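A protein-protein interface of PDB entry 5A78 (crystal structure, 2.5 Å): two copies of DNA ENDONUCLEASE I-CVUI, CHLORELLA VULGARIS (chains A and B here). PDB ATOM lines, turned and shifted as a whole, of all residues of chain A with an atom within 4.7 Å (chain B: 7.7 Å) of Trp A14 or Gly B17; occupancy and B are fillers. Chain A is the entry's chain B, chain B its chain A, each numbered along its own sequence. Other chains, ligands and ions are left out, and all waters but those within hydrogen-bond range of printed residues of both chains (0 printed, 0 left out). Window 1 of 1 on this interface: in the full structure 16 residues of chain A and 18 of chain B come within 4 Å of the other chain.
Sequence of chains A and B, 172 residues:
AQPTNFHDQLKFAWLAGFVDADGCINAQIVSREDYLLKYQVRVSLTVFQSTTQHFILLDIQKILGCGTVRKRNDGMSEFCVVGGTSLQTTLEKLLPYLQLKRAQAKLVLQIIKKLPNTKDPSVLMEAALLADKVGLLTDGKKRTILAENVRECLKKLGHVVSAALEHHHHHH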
ATOM      1  N   LEU A  10      -0.269  14.400   2.857  1.00  0.00           N
ATOM      2  CA  LEU A  10       0.612  15.469   3.306  1.00  0.00           C
ATOM      3  C   LEU A  10      -0.154  16.777   3.491  1.00  0.00           C
ATOM      4  O   LEU A  10       0.204  17.580   4.352  1.00  0.00           O
ATOM      5  CB  LEU A  10       1.774  15.673   2.327  1.00  0.00           C
ATOM      6  CG  LEU A  10       2.940  14.680   2.377  1.00  0.00           C
ATOM      7  CD1 LEU A  10       3.901  14.919   1.226  1.00  0.00           C
ATOM      8  CD2 LEU A  10       3.674  14.779   3.700  1.00  0.00           C
ATOM      9  N   LYS A  11      -1.199  16.995   2.687  1.00  0.00           N
ATOM     10  CA  LYS A  11      -2.044  18.187   2.840  1.00  0.00           C
ATOM     11  C   LYS A  11      -2.976  18.066   4.050  1.00  0.00           C
ATOM     12  O   LYS A  11      -3.244  19.050   4.745  1.00  0.00           O
ATOM     13  CB  LYS A  11      -2.872  18.456   1.574  1.00  0.00           C
ATOM     14  CG  LYS A  11      -2.058  18.939   0.367  1.00  0.00           C
ATOM     15  CD  LYS A  11      -1.636  20.413   0.508  1.00  0.00           C
ATOM     16  CE  LYS A  11      -1.956  21.239  -0.741  1.00  0.00           C
ATOM     17  NZ  LYS A  11      -2.200  22.687  -0.451  1.00  0.00           N
ATOM     18  N   PHE A  12      -3.472  16.859   4.302  1.00  0.00           N
ATOM     19  CA  PHE A  12      -4.313  16.625   5.468  1.00  0.00           C
ATOM     20  C   PHE A  12      -3.487  16.766   6.753  1.00  0.00           C
ATOM     21  O   PHE A  12      -3.974  17.272   7.766  1.00  0.00           O
ATOM     22  CB  PHE A  12      -4.973  15.247   5.390  1.00  0.00           C
ATOM     23  CG  PHE A  12      -6.060  15.156   4.357  1.00  0.00           C
ATOM     24  CD1 PHE A  12      -6.922  16.220   4.149  1.00  0.00           C
ATOM     25  CD2 PHE A  12      -6.228  14.007   3.605  1.00  0.00           C
ATOM     26  CE1 PHE A  12      -7.928  16.147   3.194  1.00  0.00           C
ATOM     27  CE2 PHE A  12      -7.229  13.925   2.644  1.00  0.00           C
ATOM     28  CZ  PHE A  12      -8.078  15.000   2.438  1.00  0.00           C
ATOM     29  N   ALA A  13      -2.231  16.335   6.696  1.00  0.00           N
ATOM     30  CA  ALA A  13      -1.323  16.487   7.832  1.00  0.00           C
ATOM     31  C   ALA A  13      -0.997  17.964   8.076  1.00  0.00           C
ATOM     32  O   ALA A  13      -0.988  18.424   9.225  1.00  0.00           O
ATOM     33  CB  ALA A  13      -0.043  15.693   7.607  1.00  0.00           C
ATOM     34  N   TRP A  14      -0.737  18.701   6.997  1.00  0.00           N
ATOM     35  CA  TRP A  14      -0.505  20.137   7.097  1.00  0.00           C
ATOM     36  C   TRP A  14      -1.750  20.802   7.650  1.00  0.00           C
ATOM     37  O   TRP A  14      -1.668  21.683   8.501  1.00  0.00           O
ATOM     38  CB  TRP A  14      -0.138  20.748   5.734  1.00  0.00           C
ATOM     39  CG  TRP A  14      -0.055  22.254   5.759  1.00  0.00           C
ATOM     40  CD1 TRP A  14       1.058  23.012   5.997  1.00  0.00           C
ATOM     41  CD2 TRP A  14      -1.131  23.182   5.554  1.00  0.00           C
ATOM     42  NE1 TRP A  14       0.741  24.348   5.956  1.00  0.00           N
ATOM     43  CE2 TRP A  14      -0.600  24.480   5.677  1.00  0.00           C
ATOM     44  CE3 TRP A  14      -2.494  23.040   5.264  1.00  0.00           C
ATOM     45  CZ2 TRP A  14      -1.378  25.631   5.533  1.00  0.00           C
ATOM     46  CZ3 TRP A  14      -3.270  24.189   5.116  1.00  0.00           C
ATOM     47  CH2 TRP A  14      -2.707  25.465   5.255  1.00  0.00           C
ATOM     48  N   LEU A  15      -2.912  20.367   7.164  1.00  0.00           N
ATOM     49  CA  LEU A  15      -4.174  20.965   7.580  1.00  0.00           C
ATOM     50  C   LEU A  15      -4.474  20.653   9.033  1.00  0.00           C
ATOM     51  O   LEU A  15      -4.904  21.525   9.796  1.00  0.00           O
ATOM     52  CB  LEU A  15      -5.329  20.493   6.699  1.00  0.00           C
ATOM     53  CG  LEU A  15      -6.630  21.146   7.167  1.00  0.00           C
ATOM     54  CD1 LEU A  15      -6.439  22.658   7.208  1.00  0.00           C
ATOM     55  CD2 LEU A  15      -7.805  20.772   6.274  1.00  0.00           C
ATOM     56  N   ALA A  16      -4.256  19.403   9.416  1.00  0.00           N
ATOM     57  CA  ALA A  16      -4.383  19.048  10.811  1.00  0.00           C
ATOM     58  C   ALA A  16      -3.446  19.944  11.616  1.00  0.00           C
ATOM     59  O   ALA A  16      -3.831  20.504  12.656  1.00  0.00           O
ATOM     60  CB  ALA A  16      -4.065  17.564  11.034  1.00  0.00           C
ATOM     61  N   GLY A  17      -2.222  20.088  11.109  1.00  0.00           N
ATOM     62  CA  GLY A  17      -1.243  20.947  11.736  1.00  0.00           C
ATOM     63  C   GLY A  17      -1.850  22.312  11.981  1.00  0.00           C
ATOM     64  O   GLY A  17      -1.777  22.839  13.086  1.00  0.00           O
ATOM     65  N   PHE A  18      -2.502  22.860  10.959  1.00  0.00           N
ATOM     66  CA  PHE A  18      -3.039  24.212  11.027  1.00  0.00           C
ATOM     67  C   PHE A  18      -4.227  24.348  11.985  1.00  0.00           C
ATOM     68  O   PHE A  18      -4.267  25.262  12.823  1.00  0.00           O
ATOM     69  CB  PHE A  18      -3.439  24.657   9.627  1.00  0.00           C
ATOM     70  CG  PHE A  18      -3.471  26.128   9.457  1.00  0.00           C
ATOM     71  CD1 PHE A  18      -2.293  26.828   9.263  1.00  0.00           C
ATOM     72  CD2 PHE A  18      -4.672  26.817   9.460  1.00  0.00           C
ATOM     73  CE1 PHE A  18      -2.296  28.196   9.088  1.00  0.00           C
ATOM     74  CE2 PHE A  18      -4.694  28.190   9.280  1.00  0.00           C
ATOM     75  CZ  PHE A  18      -3.493  28.879   9.096  1.00  0.00           C
ATOM     76  N   ILE A  56      -5.880  32.121   2.003  1.00  0.00           N
ATOM     77  CA  ILE A  56      -5.685  30.828   2.621  1.00  0.00           C
ATOM     78  C   ILE A  56      -7.018  30.208   3.005  1.00  0.00           C
ATOM     79  O   ILE A  56      -7.079  29.012   3.193  1.00  0.00           O
ATOM     80  CB  ILE A  56      -4.645  30.801   3.781  1.00  0.00           C
ATOM     81  CG1 ILE A  56      -4.052  29.415   3.939  1.00  0.00           C
ATOM     82  CG2 ILE A  56      -5.243  31.192   5.105  1.00  0.00           C
ATOM     83  CD1 ILE A  56      -2.719  29.215   3.273  1.00  0.00           C
ATOM     84  N   ILE A  60      -8.213  25.708   1.870  1.00  0.00           N
ATOM     85  CA  ILE A  60      -8.600  24.632   2.729  1.00  0.00           C
ATOM     86  C   ILE A  60      -9.889  24.010   2.258  1.00  0.00           C
ATOM     87  O   ILE A  60     -10.069  22.845   2.356  1.00  0.00           O
ATOM     88  CB  ILE A  60      -8.769  25.134   4.160  1.00  0.00           C
ATOM     89  CG1 ILE A  60      -7.430  25.577   4.726  1.00  0.00           C
ATOM     90  CG2 ILE A  60      -9.291  24.044   5.044  1.00  0.00           C
ATOM     91  CD1 ILE A  60      -7.536  26.261   6.055  1.00  0.00           C
ATOM     92  N   GLN B   9       8.065  12.996   6.926  1.00  0.00           N
ATOM     93  CA  GLN B   9       7.484  13.879   5.931  1.00  0.00           C
ATOM     94  C   GLN B   9       6.081  14.253   6.397  1.00  0.00           C
ATOM     95  O   GLN B   9       5.633  15.383   6.192  1.00  0.00           O
ATOM     96  CB  GLN B   9       7.459  13.212   4.554  1.00  0.00           C
ATOM     97  CG  GLN B   9       8.835  12.924   3.905  1.00  0.00           C
ATOM     98  CD  GLN B   9       9.943  13.959   4.205  1.00  0.00           C
ATOM     99  OE1 GLN B   9       9.719  15.175   4.175  1.00  0.00           O
ATOM    100  NE2 GLN B   9      11.152  13.463   4.471  1.00  0.00           N
ATOM    101  N   LEU B  10       5.405  13.313   7.060  1.00  0.00           N
ATOM    102  CA  LEU B  10       4.070  13.568   7.595  1.00  0.00           C
ATOM    103  C   LEU B  10       4.053  14.486   8.834  1.00  0.00           C
ATOM    104  O   LEU B  10       3.112  15.268   9.009  1.00  0.00           O
ATOM    105  CB  LEU B  10       3.373  12.239   7.904  1.00  0.00           C
ATOM    106  CG  LEU B  10       2.896  11.427   6.685  1.00  0.00           C
ATOM    107  CD1 LEU B  10       2.445  10.028   7.070  1.00  0.00           C
ATOM    108  CD2 LEU B  10       1.783  12.140   5.910  1.00  0.00           C
ATOM    109  N   LYS B  11       5.121  14.381   9.598  1.00  0.00           N
ATOM    110  CA  LYS B  11       5.359  15.103  10.817  1.00  0.00           C
ATOM    111  C   LYS B  11       5.833  16.522  10.555  1.00  0.00           C
ATOM    112  O   LYS B  11       5.490  17.429  11.266  1.00  0.00           O
ATOM    113  CB  LYS B  11       6.414  14.314  11.578  1.00  0.00           C
ATOM    114  CG  LYS B  11       6.146  14.114  13.039  1.00  0.00           C
ATOM    115  CD  LYS B  11       5.926  12.669  13.391  1.00  0.00           C
ATOM    116  CE  LYS B  11       4.622  12.523  14.157  1.00  0.00           C
ATOM    117  NZ  LYS B  11       4.499  11.227  14.870  1.00  0.00           N
ATOM    118  N   PHE B  12       6.629  16.687   9.517  1.00  0.00           N
ATOM    119  CA  PHE B  12       7.173  17.944   9.010  1.00  0.00           C
ATOM    120  C   PHE B  12       6.027  18.750   8.407  1.00  0.00           C
ATOM    121  O   PHE B  12       5.916  19.963   8.627  1.00  0.00           O
ATOM    122  CB  PHE B  12       8.261  17.723   7.951  1.00  0.00           C
ATOM    123  CG  PHE B  12       9.563  17.199   8.492  1.00  0.00           C
ATOM    124  CD1 PHE B  12       9.847  17.244   9.850  1.00  0.00           C
ATOM    125  CD2 PHE B  12      10.520  16.682   7.626  1.00  0.00           C
ATOM    126  CE1 PHE B  12      11.059  16.762  10.341  1.00  0.00           C
ATOM    127  CE2 PHE B  12      11.725  16.204   8.105  1.00  0.00           C
ATOM    128  CZ  PHE B  12      11.996  16.243   9.469  1.00  0.00           C
ATOM    129  N   ALA B  13       5.180  18.059   7.641  1.00  0.00           N
ATOM    130  CA  ALA B  13       4.003  18.675   7.041  1.00  0.00           C
ATOM    131  C   ALA B  13       3.055  19.151   8.131  1.00  0.00           C
ATOM    132  O   ALA B  13       2.524  20.264   8.062  1.00  0.00           O
ATOM    133  CB  ALA B  13       3.292  17.697   6.109  1.00  0.00           C
ATOM    134  N   TRP B  14       2.850  18.305   9.137  1.00  0.00           N
ATOM    135  CA  TRP B  14       2.016  18.681  10.257  1.00  0.00           C
ATOM    136  C   TRP B  14       2.625  19.921  10.900  1.00  0.00           C
ATOM    137  O   TRP B  14       1.941  20.930  11.078  1.00  0.00           O
ATOM    138  CB  TRP B  14       1.884  17.529  11.273  1.00  0.00           C
ATOM    139  CG  TRP B  14       1.130  17.935  12.495  1.00  0.00           C
ATOM    140  CD1 TRP B  14      -0.228  17.882  12.686  1.00  0.00           C
ATOM    141  CD2 TRP B  14       1.683  18.488  13.691  1.00  0.00           C
ATOM    142  NE1 TRP B  14      -0.547  18.365  13.934  1.00  0.00           N
ATOM    143  CE2 TRP B  14       0.612  18.739  14.573  1.00  0.00           C
ATOM    144  CE3 TRP B  14       2.986  18.789  14.110  1.00  0.00           C
ATOM    145  CZ2 TRP B  14       0.800  19.284  15.838  1.00  0.00           C
ATOM    146  CZ3 TRP B  14       3.175  19.330  15.363  1.00  0.00           C
ATOM    147  CH2 TRP B  14       2.085  19.574  16.212  1.00  0.00           C
ATOM    148  N   LEU B  15       3.919  19.852  11.204  1.00  0.00           N
ATOM    149  CA  LEU B  15       4.651  20.976  11.801  1.00  0.00           C
ATOM    150  C   LEU B  15       4.537  22.263  10.989  1.00  0.00           C
ATOM    151  O   LEU B  15       4.264  23.333  11.542  1.00  0.00           O
ATOM    152  CB  LEU B  15       6.132  20.626  11.970  1.00  0.00           C
ATOM    153  CG  LEU B  15       6.934  21.611  12.818  1.00  0.00           C
ATOM    154  CD1 LEU B  15       6.149  21.944  14.083  1.00  0.00           C
ATOM    155  CD2 LEU B  15       8.327  21.063  13.164  1.00  0.00           C
ATOM    156  N   ALA B  16       4.757  22.166   9.680  1.00  0.00           N
ATOM    157  CA  ALA B  16       4.626  23.328   8.812  1.00  0.00           C
ATOM    158  C   ALA B  16       3.228  23.939   8.932  1.00  0.00           C
ATOM    159  O   ALA B  16       3.066  25.168   8.891  1.00  0.00           O
ATOM    160  CB  ALA B  16       4.922  22.951   7.366  1.00  0.00           C
ATOM    161  N   GLY B  17       2.223  23.072   9.090  1.00  0.00           N
ATOM    162  CA  GLY B  17       0.858  23.512   9.304  1.00  0.00           C
ATOM    163  C   GLY B  17       0.748  24.283  10.605  1.00  0.00           C
ATOM    164  O   GLY B  17       0.110  25.331  10.675  1.00  0.00           O
ATOM    165  N   PHE B  18       1.398  23.780  11.640  1.00  0.00           N
ATOM    166  CA  PHE B  18       1.372  24.465  12.921  1.00  0.00           C
ATOM    167  C   PHE B  18       2.116  25.809  12.847  1.00  0.00           C
ATOM    168  O   PHE B  18       1.541  26.861  13.161  1.00  0.00           O
ATOM    169  CB  PHE B  18       1.967  23.566  14.000  1.00  0.00           C
ATOM    170  CG  PHE B  18       1.447  23.836  15.365  1.00  0.00           C
ATOM    171  CD1 PHE B  18       0.231  23.284  15.770  1.00  0.00           C
ATOM    172  CD2 PHE B  18       2.171  24.604  16.265  1.00  0.00           C
ATOM    173  CE1 PHE B  18      -0.271  23.506  17.052  1.00  0.00           C
ATOM    174  CE2 PHE B  18       1.692  24.832  17.553  1.00  0.00           C
ATOM    175  CZ  PHE B  18       0.463  24.280  17.951  1.00  0.00           C
ATOM    176  N   VAL B  19       3.387  25.772  12.436  1.00  0.00           N
ATOM    177  CA  VAL B  19       4.187  26.993  12.246  1.00  0.00           C
ATOM    178  C   VAL B  19       3.428  28.063  11.429  1.00  0.00           C
ATOM    179  O   VAL B  19       3.393  29.239  11.811  1.00  0.00           O
ATOM    180  CB  VAL B  19       5.541  26.689  11.537  1.00  0.00           C
ATOM    181  CG1 VAL B  19       6.183  27.966  11.018  1.00  0.00           C
ATOM    182  CG2 VAL B  19       6.493  25.956  12.461  1.00  0.00           C
ATOM    183  N   ASP B  20       2.814  27.665  10.320  1.00  0.00           N
ATOM    184  CA  ASP B  20       2.075  28.637   9.520  1.00  0.00           C
ATOM    185  C   ASP B  20       0.953  29.311  10.311  1.00  0.00           C
ATOM    186  O   ASP B  20       0.625  30.483  10.078  1.00  0.00           O
ATOM    187  CB  ASP B  20       1.500  27.978   8.260  1.00  0.00           C
ATOM    188  CG  ASP B  20       2.387  28.182   7.047  1.00  0.00           C
ATOM    189  OD1 ASP B  20       3.229  29.105   7.092  1.00  0.00           O
ATOM    190  OD2 ASP B  20       2.252  27.429   6.059  1.00  0.00           O
ATOM    191  N   ALA B  21       0.371  28.568  11.249  1.00  0.00           N
ATOM    192  CA  ALA B  21      -0.723  29.087  12.052  1.00  0.00           C
ATOM    193  C   ALA B  21      -0.235  29.924  13.235  1.00  0.00           C
ATOM    194  O   ALA B  21      -0.579  31.099  13.334  1.00  0.00           O
ATOM    195  CB  ALA B  21      -1.594  27.941  12.540  1.00  0.00           C
ATOM    196  N   ASP B  22       0.549  29.328  14.137  1.00  0.00           N
ATOM    197  CA  ASP B  22       0.955  30.031  15.359  1.00  0.00           C
ATOM    198  C   ASP B  22       2.473  30.029  15.521  1.00  0.00           C
ATOM    199  O   ASP B  22       2.997  29.741  16.612  1.00  0.00           O
ATOM    200  CB  ASP B  22       0.324  29.411  16.607  1.00  0.00           C
ATOM    201  CG  ASP B  22      -1.204  29.459  16.581  1.00  0.00           C
ATOM    202  OD1 ASP B  22      -1.768  30.092  15.652  1.00  0.00           O
ATOM    203  OD2 ASP B  22      -1.842  28.886  17.503  1.00  0.00           O
ATOM    204  N   GLY B  23       3.165  30.346  14.430  1.00  0.00           N
ATOM    205  CA  GLY B  23       4.608  30.338  14.419  1.00  0.00           C
ATOM    206  C   GLY B  23       5.183  31.728  14.278  1.00  0.00           C
ATOM    207  O   GLY B  23       4.484  32.728  14.394  1.00  0.00           O
ATOM    208  N   LEU B  94      10.969  22.275   6.781  1.00  0.00           N
ATOM    209  CA  LEU B  94       9.649  22.743   6.588  1.00  0.00           C
ATOM    210  C   LEU B  94       9.452  23.207   5.141  1.00  0.00           C
ATOM    211  O   LEU B  94       8.484  22.915   4.499  1.00  0.00           O
ATOM    212  CB  LEU B  94       9.380  23.868   7.574  1.00  0.00           C
ATOM    213  CG  LEU B  94       9.751  23.516   8.993  1.00  0.00           C
ATOM    214  CD1 LEU B  94       9.430  24.610   9.972  1.00  0.00           C
ATOM    215  CD2 LEU B  94       9.039  22.252   9.380  1.00  0.00           C
ATOM    216  N   PRO B  96       9.493  22.764   2.121  1.00  0.00           N
ATOM    217  CA  PRO B  96       8.578  22.250   1.095  1.00  0.00           C
ATOM    218  C   PRO B  96       7.105  22.329   1.503  1.00  0.00           C
ATOM    219  O   PRO B  96       6.255  22.380   0.620  1.00  0.00           O
ATOM    220  CB  PRO B  96       9.014  20.790   0.933  1.00  0.00           C
ATOM    221  CG  PRO B  96      10.428  20.752   1.418  1.00  0.00           C
ATOM    222  CD  PRO B  96      10.467  21.740   2.549  1.00  0.00           C
ATOM    223  N   TYR B  97       6.804  22.359   2.800  1.00  0.00           N
ATOM    224  CA  TYR B  97       5.409  22.322   3.237  1.00  0.00           C
ATOM    225  C   TYR B  97       4.902  23.665   3.740  1.00  0.00           C
ATOM    226  O   TYR B  97       3.697  23.872   3.851  1.00  0.00           O
ATOM    227  CB  TYR B  97       5.211  21.256   4.319  1.00  0.00           C
ATOM    228  CG  TYR B  97       5.779  19.924   3.913  1.00  0.00           C
ATOM    229  CD1 TYR B  97       5.285  19.254   2.798  1.00  0.00           C
ATOM    230  CD2 TYR B  97       6.821  19.345   4.624  1.00  0.00           C
ATOM    231  CE1 TYR B  97       5.809  18.037   2.406  1.00  0.00           C
ATOM    232  CE2 TYR B  97       7.351  18.126   4.244  1.00  0.00           C
ATOM    233  CZ  TYR B  97       6.839  17.475   3.137  1.00  0.00           C
ATOM    234  OH  TYR B  97       7.363  16.258   2.754  1.00  0.00           O
ATOM    235  N   LEU B  98       5.769  24.591   4.004  1.00  0.00           N
ATOM    236  CA  LEU B  98       5.249  25.844   4.411  1.00  0.00           C
ATOM    237  C   LEU B  98       4.452  26.479   3.323  1.00  0.00           C
ATOM    238  O   LEU B  98       4.669  26.238   2.178  1.00  0.00           O
ATOM    239  CB  LEU B  98       6.360  26.770   4.777  1.00  0.00           C
ATOM    240  CG  LEU B  98       7.161  26.360   5.965  1.00  0.00           C
ATOM    241  CD1 LEU B  98       8.317  27.325   6.093  1.00  0.00           C
ATOM    242  CD2 LEU B  98       6.194  26.552   7.096  1.00  0.00           C
ATOM    243  N   GLN B  99       3.539  27.336   3.718  1.00  0.00           N
ATOM    244  CA  GLN B  99       2.673  28.063   2.804  1.00  0.00           C
ATOM    245  C   GLN B  99       2.716  29.535   3.135  1.00  0.00           C
ATOM    246  O   GLN B  99       3.335  30.336   2.429  1.00  0.00           O
ATOM    247  CB  GLN B  99       1.241  27.559   2.916  1.00  0.00           C
ATOM    248  CG  GLN B  99       1.081  26.120   2.511  1.00  0.00           C
ATOM    249  CD  GLN B  99       1.342  25.920   1.044  1.00  0.00           C
ATOM    250  OE1 GLN B  99       0.851  26.681   0.203  1.00  0.00           O
ATOM    251  NE2 GLN B  99       2.137  24.910   0.719  1.00  0.00           N
ATOM    252  N   LEU B 100       2.057  29.864   4.241  1.00  0.00           N
ATOM    253  CA  LEU B 100       1.882  31.230   4.704  1.00  0.00           C
ATOM    254  C   LEU B 100       3.178  31.971   4.969  1.00  0.00           C
ATOM    255  O   LEU B 100       3.246  33.193   4.784  1.00  0.00           O
ATOM    256  CB  LEU B 100       1.045  31.235   5.978  1.00  0.00           C
ATOM    257  CG  LEU B 100      -0.421  30.915   5.753  1.00  0.00           C
ATOM    258  CD1 LEU B 100      -1.189  31.144   7.038  1.00  0.00           C
ATOM    259  CD2 LEU B 100      -0.938  31.797   4.629  1.00  0.00           C
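OD2 of Asp B20 lies within hydrogen-bond range of NE1 of Trp A14 (3.4 Å).
The side-chain hydroxyl (OH) of Tyr B97 is in hydrogen-bond range of the side-chain amide oxygen (OE1) of Gln B9 (3.0 Å).
N of Gln B99 sits at hydrogen-bond distance from OD2 of Asp B20, 2.7 Å away.
OD2 of Asp B20 lies within hydrogen-bond range of N of Leu B100 (3.0 Å).
CD2 of Leu A10 touches O of Gln B9, at 3.2 Å.
Leu B10 touches Leu A10 (CD2 to CD2, 3.9 Å).
Leu A10 touches Ala B13.
Leu A10 touches Tyr B97.
Trp B14 touches Ala A13 (CA to O, 3.2 Å).
Gly A17 touches Gly B17.
O of Gly A17 touches CD1 of Phe B18, 3.4 Å away.
O of Gly B17 touches CD1 of Phe A18 (3.2 Å).
Asp B20 touches Phe A18 (C to CE1, 3.6 Å).
Phe A18 touches Ala B21 (CE1 to N, 3.5 Å).
Trp A14 touches six residues of chain B.
Printed residues of chain A within 4 Å of Gly B17: Trp A14 (3.2 Å), Gly A17 (3.5 Å) and Phe A18 (3.2 Å).
Of the printed residues of chain A, Ala B21 touches Phe A18 (3.5 Å).
Of the printed residues of chain A, Asp B20 touches Trp A14 (3.4 Å) and Phe A18 (3.6 Å).
Of the printed residues of chain A, Gln B9 touches Leu A10.
Printed residues of chain A within 4 Å of Leu B10: Leu A10 and Ala A13.
Of the printed residues of chain A, Tyr B97 touches Leu A10 and Trp A14.
Lys B11 touches none of the printed residues of chain A.
The nearest printed residue of chain A that does not touch Gly B17 is Leu A15 (5.4 Å).
The nearest printed residue of chain B that does not touch Ile A56 is Gln B99 (4.3 Å).
Printed residues of chain A that touch a printed residue of chain B: Leu A10, Ala A13, Trp A14, Ala A16, Gly A17, Phe A18 and Ile A56.
Of the 21 printed residues of chain B, 12 touch a printed residue of chain A.
Hydrophobic or aromatic side chains of chain B that line the printed part of chain A: Leu B10, Ala B13, Trp B14, Phe B18, Ala B21, Tyr B97 and Leu B100.
Among the printed residues, no Asp or Glu carboxylate lies within 4 Å of a Lys or Arg side-chain nitrogen of the other chain.
Leu A10 touches Ala B13, and with the chains exchanged Ala A13 touches Leu B10.
Ala A13 touches Trp B14, and with the chains exchanged Trp A14 touches Ala B13.
Trp A14 touches Ala B16, and with the chains exchanged Ala A16 touches Trp B14.
Trp A14 touches Gly B17, and with the chains exchanged Gly A17 touches Trp B14.
9 positions are printed for both chains.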
